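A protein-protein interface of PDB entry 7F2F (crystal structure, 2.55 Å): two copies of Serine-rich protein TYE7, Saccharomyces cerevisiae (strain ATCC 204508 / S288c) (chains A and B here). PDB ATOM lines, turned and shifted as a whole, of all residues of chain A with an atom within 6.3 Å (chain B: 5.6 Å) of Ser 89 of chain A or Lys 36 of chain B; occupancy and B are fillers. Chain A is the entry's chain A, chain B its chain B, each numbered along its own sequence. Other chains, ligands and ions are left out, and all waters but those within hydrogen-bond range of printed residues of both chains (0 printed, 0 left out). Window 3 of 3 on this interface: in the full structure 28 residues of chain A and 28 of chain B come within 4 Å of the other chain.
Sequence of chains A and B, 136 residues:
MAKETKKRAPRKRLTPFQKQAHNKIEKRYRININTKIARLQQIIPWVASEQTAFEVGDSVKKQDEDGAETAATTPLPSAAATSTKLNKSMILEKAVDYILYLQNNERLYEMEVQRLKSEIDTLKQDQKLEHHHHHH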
ATOM      1  N   ASN A  87     -10.664 -15.572   0.350  1.00  0.00           N
ATOM      2  CA  ASN A  87     -11.253 -15.261  -0.935  1.00  0.00           C
ATOM      3  C   ASN A  87     -10.736 -13.972  -1.502  1.00  0.00           C
ATOM      4  O   ASN A  87     -10.209 -13.117  -0.814  1.00  0.00           O
ATOM      5  CB  ASN A  87     -12.765 -15.060  -0.809  1.00  0.00           C
ATOM      6  CG  ASN A  87     -13.401 -16.043   0.144  1.00  0.00           C
ATOM      7  OD1 ASN A  87     -13.430 -17.263  -0.115  1.00  0.00           O
ATOM      8  ND2 ASN A  87     -13.888 -15.526   1.279  1.00  0.00           N
ATOM      9  N   LYS A  88     -11.039 -13.776  -2.762  1.00  0.00           N
ATOM     10  CA  LYS A  88     -10.555 -12.640  -3.476  1.00  0.00           C
ATOM     11  C   LYS A  88     -10.926 -11.356  -2.795  1.00  0.00           C
ATOM     12  O   LYS A  88     -10.051 -10.512  -2.536  1.00  0.00           O
ATOM     13  CB  LYS A  88     -11.035 -12.658  -4.935  1.00  0.00           C
ATOM     14  CG  LYS A  88     -10.366 -13.798  -5.701  1.00  0.00           C
ATOM     15  CD  LYS A  88     -10.939 -14.007  -7.084  1.00  0.00           C
ATOM     16  CE  LYS A  88     -10.328 -15.277  -7.645  1.00  0.00           C
ATOM     17  NZ  LYS A  88     -11.054 -15.688  -8.884  1.00  0.00           N
ATOM     18  N   SER A  89     -12.197 -11.210  -2.471  1.00  0.00           N
ATOM     19  CA  SER A  89     -12.675  -9.920  -1.977  1.00  0.00           C
ATOM     20  C   SER A  89     -12.086  -9.650  -0.577  1.00  0.00           C
ATOM     21  O   SER A  89     -11.863  -8.526  -0.239  1.00  0.00           O
ATOM     22  CB  SER A  89     -14.183  -9.864  -1.975  1.00  0.00           C
ATOM     23  OG  SER A  89     -14.639 -11.036  -1.344  1.00  0.00           O
ATOM     24  N   MET A  90     -11.770 -10.699   0.172  1.00  0.00           N
ATOM     25  CA  MET A  90     -11.197 -10.561   1.481  1.00  0.00           C
ATOM     26  C   MET A  90      -9.828  -9.923   1.344  1.00  0.00           C
ATOM     27  O   MET A  90      -9.497  -8.955   2.066  1.00  0.00           O
ATOM     28  CB  MET A  90     -11.097 -11.928   2.174  1.00  0.00           C
ATOM     29  CG  MET A  90     -10.681 -11.919   3.628  1.00  0.00           C
ATOM     30  SD  MET A  90     -11.734 -10.893   4.699  1.00  0.00           S
ATOM     31  CE  MET A  90     -10.915 -11.096   6.300  1.00  0.00           C
ATOM     32  N   ILE A  91      -9.054 -10.443   0.397  1.00  0.00           N
ATOM     33  CA  ILE A  91      -7.742  -9.908   0.124  1.00  0.00           C
ATOM     34  C   ILE A  91      -7.826  -8.467  -0.362  1.00  0.00           C
ATOM     35  O   ILE A  91      -7.112  -7.593   0.146  1.00  0.00           O
ATOM     36  CB  ILE A  91      -7.001 -10.792  -0.835  1.00  0.00           C
ATOM     37  CG1 ILE A  91      -6.582 -12.054  -0.068  1.00  0.00           C
ATOM     38  CG2 ILE A  91      -5.780 -10.075  -1.388  1.00  0.00           C
ATOM     39  CD1 ILE A  91      -6.243 -13.202  -0.976  1.00  0.00           C
ATOM     40  N   LEU A  92      -8.770  -8.171  -1.226  1.00  0.00           N
ATOM     41  CA  LEU A  92      -8.967  -6.780  -1.602  1.00  0.00           C
ATOM     42  C   LEU A  92      -9.304  -5.839  -0.418  1.00  0.00           C
ATOM     43  O   LEU A  92      -8.643  -4.784  -0.296  1.00  0.00           O
ATOM     44  CB  LEU A  92      -9.997  -6.696  -2.732  1.00  0.00           C
ATOM     45  CG  LEU A  92      -9.563  -7.404  -4.052  1.00  0.00           C
ATOM     46  CD1 LEU A  92     -10.697  -7.577  -5.082  1.00  0.00           C
ATOM     47  CD2 LEU A  92      -8.340  -6.746  -4.702  1.00  0.00           C
ATOM     48  N   GLU A  93     -10.275  -6.224   0.458  1.00  0.00           N
ATOM     49  CA  GLU A  93     -10.679  -5.403   1.564  1.00  0.00           C
ATOM     50  C   GLU A  93      -9.497  -5.222   2.489  1.00  0.00           C
ATOM     51  O   GLU A  93      -9.293  -4.146   2.953  1.00  0.00           O
ATOM     52  CB  GLU A  93     -11.808  -6.014   2.428  1.00  0.00           C
ATOM     53  CG  GLU A  93     -13.172  -6.020   1.798  1.00  0.00           C
ATOM     54  CD  GLU A  93     -13.887  -4.672   1.743  1.00  0.00           C
ATOM     55  OE1 GLU A  93     -13.643  -3.874   0.771  1.00  0.00           O
ATOM     56  OE2 GLU A  93     -14.772  -4.464   2.622  1.00  0.00           O
ATOM     57  N   LYS A  94      -8.772  -6.297   2.794  1.00  0.00           N
ATOM     58  CA  LYS A  94      -7.662  -6.222   3.691  1.00  0.00           C
ATOM     59  C   LYS A  94      -6.588  -5.319   3.120  1.00  0.00           C
ATOM     60  O   LYS A  94      -6.026  -4.518   3.866  1.00  0.00           O
ATOM     61  CB  LYS A  94      -7.088  -7.596   3.986  1.00  0.00           C
ATOM     62  CG  LYS A  94      -8.017  -8.501   4.791  1.00  0.00           C
ATOM     63  CD  LYS A  94      -8.051  -8.276   6.315  1.00  0.00           C
ATOM     64  CE  LYS A  94      -9.218  -7.373   6.734  1.00  0.00           C
ATOM     65  NZ  LYS A  94      -8.807  -6.338   7.747  1.00  0.00           N
ATOM     66  N   VAL A  96      -6.961  -2.749   1.203  1.00  0.00           N
ATOM     67  CA  VAL A  96      -7.352  -1.379   1.544  1.00  0.00           C
ATOM     68  C   VAL A  96      -7.200  -1.122   3.059  1.00  0.00           C
ATOM     69  O   VAL A  96      -6.789  -0.030   3.453  1.00  0.00           O
ATOM     70  CB  VAL A  96      -8.804  -1.065   1.178  1.00  0.00           C
ATOM     71  CG1 VAL A  96      -9.126   0.358   1.551  1.00  0.00           C
ATOM     72  CG2 VAL A  96      -9.077  -1.257  -0.309  1.00  0.00           C
ATOM     73  N   ILE B  31     -19.435  -7.120  -9.979  1.00  0.00           N
ATOM     74  CA  ILE B  31     -19.285  -5.689  -9.575  1.00  0.00           C
ATOM     75  C   ILE B  31     -18.814  -5.519  -8.129  1.00  0.00           C
ATOM     76  O   ILE B  31     -18.266  -4.481  -7.795  1.00  0.00           O
ATOM     77  CB  ILE B  31     -20.527  -4.785  -9.755  1.00  0.00           C
ATOM     78  CG1 ILE B  31     -21.766  -5.436  -9.120  1.00  0.00           C
ATOM     79  CG2 ILE B  31     -20.639  -4.297 -11.219  1.00  0.00           C
ATOM     80  CD1 ILE B  31     -22.978  -5.550 -10.032  1.00  0.00           C
ATOM     81  N   ASN B  32     -18.993  -6.529  -7.283  1.00  0.00           N
ATOM     82  CA  ASN B  32     -18.427  -6.461  -5.971  1.00  0.00           C
ATOM     83  C   ASN B  32     -16.896  -6.466  -6.115  1.00  0.00           C
ATOM     84  O   ASN B  32     -16.236  -5.563  -5.559  1.00  0.00           O
ATOM     85  CB  ASN B  32     -18.959  -7.551  -5.018  1.00  0.00           C
ATOM     86  CG  ASN B  32     -18.416  -7.403  -3.600  1.00  0.00           C
ATOM     87  OD1 ASN B  32     -18.441  -6.308  -3.026  1.00  0.00           O
ATOM     88  ND2 ASN B  32     -17.890  -8.494  -3.038  1.00  0.00           N
ATOM     89  N   ILE B  33     -16.352  -7.416  -6.890  1.00  0.00           N
ATOM     90  CA  ILE B  33     -14.923  -7.437  -7.171  1.00  0.00           C
ATOM     91  C   ILE B  33     -14.516  -6.138  -7.860  1.00  0.00           C
ATOM     92  O   ILE B  33     -13.555  -5.478  -7.483  1.00  0.00           O
ATOM     93  CB  ILE B  33     -14.464  -8.597  -8.035  1.00  0.00           C
ATOM     94  CG1 ILE B  33     -14.767  -9.948  -7.385  1.00  0.00           C
ATOM     95  CG2 ILE B  33     -12.968  -8.529  -8.269  1.00  0.00           C
ATOM     96  CD1 ILE B  33     -14.288 -10.101  -5.975  1.00  0.00           C
ATOM     97  N   ASN B  34     -15.265  -5.684  -8.817  1.00  0.00           N
ATOM     98  CA  ASN B  34     -14.738  -4.508  -9.484  1.00  0.00           C
ATOM     99  C   ASN B  34     -14.607  -3.334  -8.543  1.00  0.00           C
ATOM    100  O   ASN B  34     -13.670  -2.558  -8.675  1.00  0.00           O
ATOM    101  CB  ASN B  34     -15.567  -4.123 -10.688  1.00  0.00           C
ATOM    102  CG  ASN B  34     -15.407  -5.084 -11.836  1.00  0.00           C
ATOM    103  OD1 ASN B  34     -14.695  -6.092 -11.759  1.00  0.00           O
ATOM    104  ND2 ASN B  34     -16.091  -4.770 -12.937  1.00  0.00           N
ATOM    105  N   THR B  35     -15.533  -3.198  -7.610  1.00  0.00           N
ATOM    106  CA  THR B  35     -15.572  -2.008  -6.749  1.00  0.00           C
ATOM    107  C   THR B  35     -14.458  -2.085  -5.733  1.00  0.00           C
ATOM    108  O   THR B  35     -13.869  -1.088  -5.421  1.00  0.00           O
ATOM    109  CB  THR B  35     -16.904  -1.883  -6.001  1.00  0.00           C
ATOM    110  OG1 THR B  35     -17.224  -3.171  -5.466  1.00  0.00           O
ATOM    111  CG2 THR B  35     -18.058  -1.462  -6.965  1.00  0.00           C
ATOM    112  N   LYS B  36     -14.139  -3.284  -5.265  1.00  0.00           N
ATOM    113  CA  LYS B  36     -13.012  -3.456  -4.402  1.00  0.00           C
ATOM    114  C   LYS B  36     -11.720  -3.132  -5.135  1.00  0.00           C
ATOM    115  O   LYS B  36     -10.862  -2.431  -4.581  1.00  0.00           O
ATOM    116  CB  LYS B  36     -12.980  -4.836  -3.763  1.00  0.00           C
ATOM    117  CG  LYS B  36     -14.164  -5.072  -2.855  1.00  0.00           C
ATOM    118  CD  LYS B  36     -14.047  -6.354  -2.054  1.00  0.00           C
ATOM    119  CE  LYS B  36     -15.351  -6.671  -1.309  1.00  0.00           C
ATOM    120  NZ  LYS B  36     -15.883  -5.559  -0.477  1.00  0.00           N
ATOM    121  N   ILE B  37     -11.607  -3.550  -6.386  1.00  0.00           N
ATOM    122  CA  ILE B  37     -10.475  -3.153  -7.172  1.00  0.00           C
ATOM    123  C   ILE B  37     -10.395  -1.637  -7.380  1.00  0.00           C
ATOM    124  O   ILE B  37      -9.336  -1.051  -7.251  1.00  0.00           O
ATOM    125  CB  ILE B  37     -10.346  -3.930  -8.449  1.00  0.00           C
ATOM    126  CG1 ILE B  37      -9.999  -5.357  -8.087  1.00  0.00           C
ATOM    127  CG2 ILE B  37      -9.154  -3.381  -9.245  1.00  0.00           C
ATOM    128  CD1 ILE B  37     -10.106  -6.337  -9.230  1.00  0.00           C
ATOM    129  N   ALA B  38     -11.507  -0.990  -7.615  1.00  0.00           N
ATOM    130  CA  ALA B  38     -11.481   0.438  -7.754  1.00  0.00           C
ATOM    131  C   ALA B  38     -11.187   1.186  -6.457  1.00  0.00           C
ATOM    132  O   ALA B  38     -10.592   2.262  -6.468  1.00  0.00           O
ATOM    133  CB  ALA B  38     -12.800   0.895  -8.305  1.00  0.00           C
ATOM    134  N   ARG B  39     -11.657   0.659  -5.344  1.00  0.00           N
ATOM    135  CA  ARG B  39     -11.389   1.277  -4.056  1.00  0.00           C
ATOM    136  C   ARG B  39      -9.908   1.214  -3.820  1.00  0.00           C
ATOM    137  O   ARG B  39      -9.335   2.148  -3.317  1.00  0.00           O
ATOM    138  CB  ARG B  39     -12.162   0.603  -2.880  1.00  0.00           C
ATOM    139  CG  ARG B  39     -13.413   1.371  -2.471  1.00  0.00           C
ATOM    140  CD  ARG B  39     -13.917   0.994  -1.098  1.00  0.00           C
ATOM    141  NE  ARG B  39     -14.434  -0.361  -1.116  1.00  0.00           N
ATOM    142  CZ  ARG B  39     -15.648  -0.687  -1.512  1.00  0.00           C
ATOM    143  NH1 ARG B  39     -16.013  -1.971  -1.485  1.00  0.00           N
ATOM    144  NH2 ARG B  39     -16.505   0.265  -1.910  1.00  0.00           N
ATOM    145  N   LEU B  40      -9.300   0.112  -4.190  1.00  0.00           N
ATOM    146  CA  LEU B  40      -7.898  -0.049  -3.969  1.00  0.00           C
ATOM    147  C   LEU B  40      -7.172   0.927  -4.854  1.00  0.00           C
ATOM    148  O   LEU B  40      -6.236   1.594  -4.422  1.00  0.00           O
ATOM    149  CB  LEU B  40      -7.497  -1.469  -4.307  1.00  0.00           C
ATOM    150  CG  LEU B  40      -6.070  -1.887  -4.121  1.00  0.00           C
ATOM    151  CD1 LEU B  40      -5.529  -1.381  -2.804  1.00  0.00           C
ATOM    152  CD2 LEU B  40      -5.972  -3.409  -4.181  1.00  0.00           C
ATOM    153  N   GLN B  41      -7.632   1.091  -6.083  1.00  0.00           N
ATOM    154  CA  GLN B  41      -6.973   2.062  -6.960  1.00  0.00           C
ATOM    155  C   GLN B  41      -7.073   3.443  -6.314  1.00  0.00           C
ATOM    156  O   GLN B  41      -6.144   4.246  -6.381  1.00  0.00           O
ATOM    157  CB  GLN B  41      -7.608   2.077  -8.339  1.00  0.00           C
ATOM    158  CG  GLN B  41      -7.316   3.314  -9.212  1.00  0.00           C
ATOM    159  CD  GLN B  41      -8.387   3.616 -10.256  1.00  0.00           C
ATOM    160  OE1 GLN B  41      -9.319   2.837 -10.452  1.00  0.00           O
ATOM    161  NE2 GLN B  41      -8.255   4.749 -10.922  1.00  0.00           N
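Printed residues of chain B within 4 Å of Ser 89 of chain A: Lys 36. Of the printed residues of chain B, Glu 93 of chain A touches Lys 36 and Arg 39. Of the printed residues of chain B, Leu 92 of chain A touches Lys 36 and Ile 37. Printed residues of chain A within 4 Å of Arg 39 of chain B: Glu 93. Lys 88 of chain A touches none of the printed residues of chain B. Ile 31 of chain B touches none of the printed residues of chain A. The nearest printed residue of chain B that does not touch Ser 89 of chain A is Ile 33 of chain B (4.01 Å). The nearest residue of chain A that does not touch Lys 36 of chain B is Val 96 of chain A (4.8 Å).
Of the 9 printed residues of chain A, 3 touch a printed residue of chain B. Hydrophobic or aromatic side chains of chain A within 4 Å of the printed part of chain B: Leu 92. Of the 11 printed residues of chain B, 3 touch a printed residue of chain A. Printed residues of chain B that touch a printed residue of chain A: Lys 36, Ile 37 and Arg 39. Among the printed residues, Asp or Glu carboxylates within 4 Å of a Lys or Arg side-chain nitrogen of the other chain: Glu 93 of chain A with Lys 36 of chain B and Glu 93 of chain A with Arg 39 of chain B.
The side-chain amino group of Lys 36 of chain B lies within salt-bridge range of the side-chain carboxylate of Glu 93 of chain A (3.1 Å). The guanidinium group of Arg 39 of chain B lies within salt-bridge range of the side-chain carboxylate of Glu 93 of chain A.
No position is printed for both chains.
CB of Ser 89 of chain A touches CE of Lys 36 of chain B, at 3.5 Å. Leu 92 of chain A touches Lys 36 of chain B (CB to CB, 3.7 Å). CD1 of Leu 92 of chain A touches CG1 of Ile 37 of chain B, 3.8 Å away.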
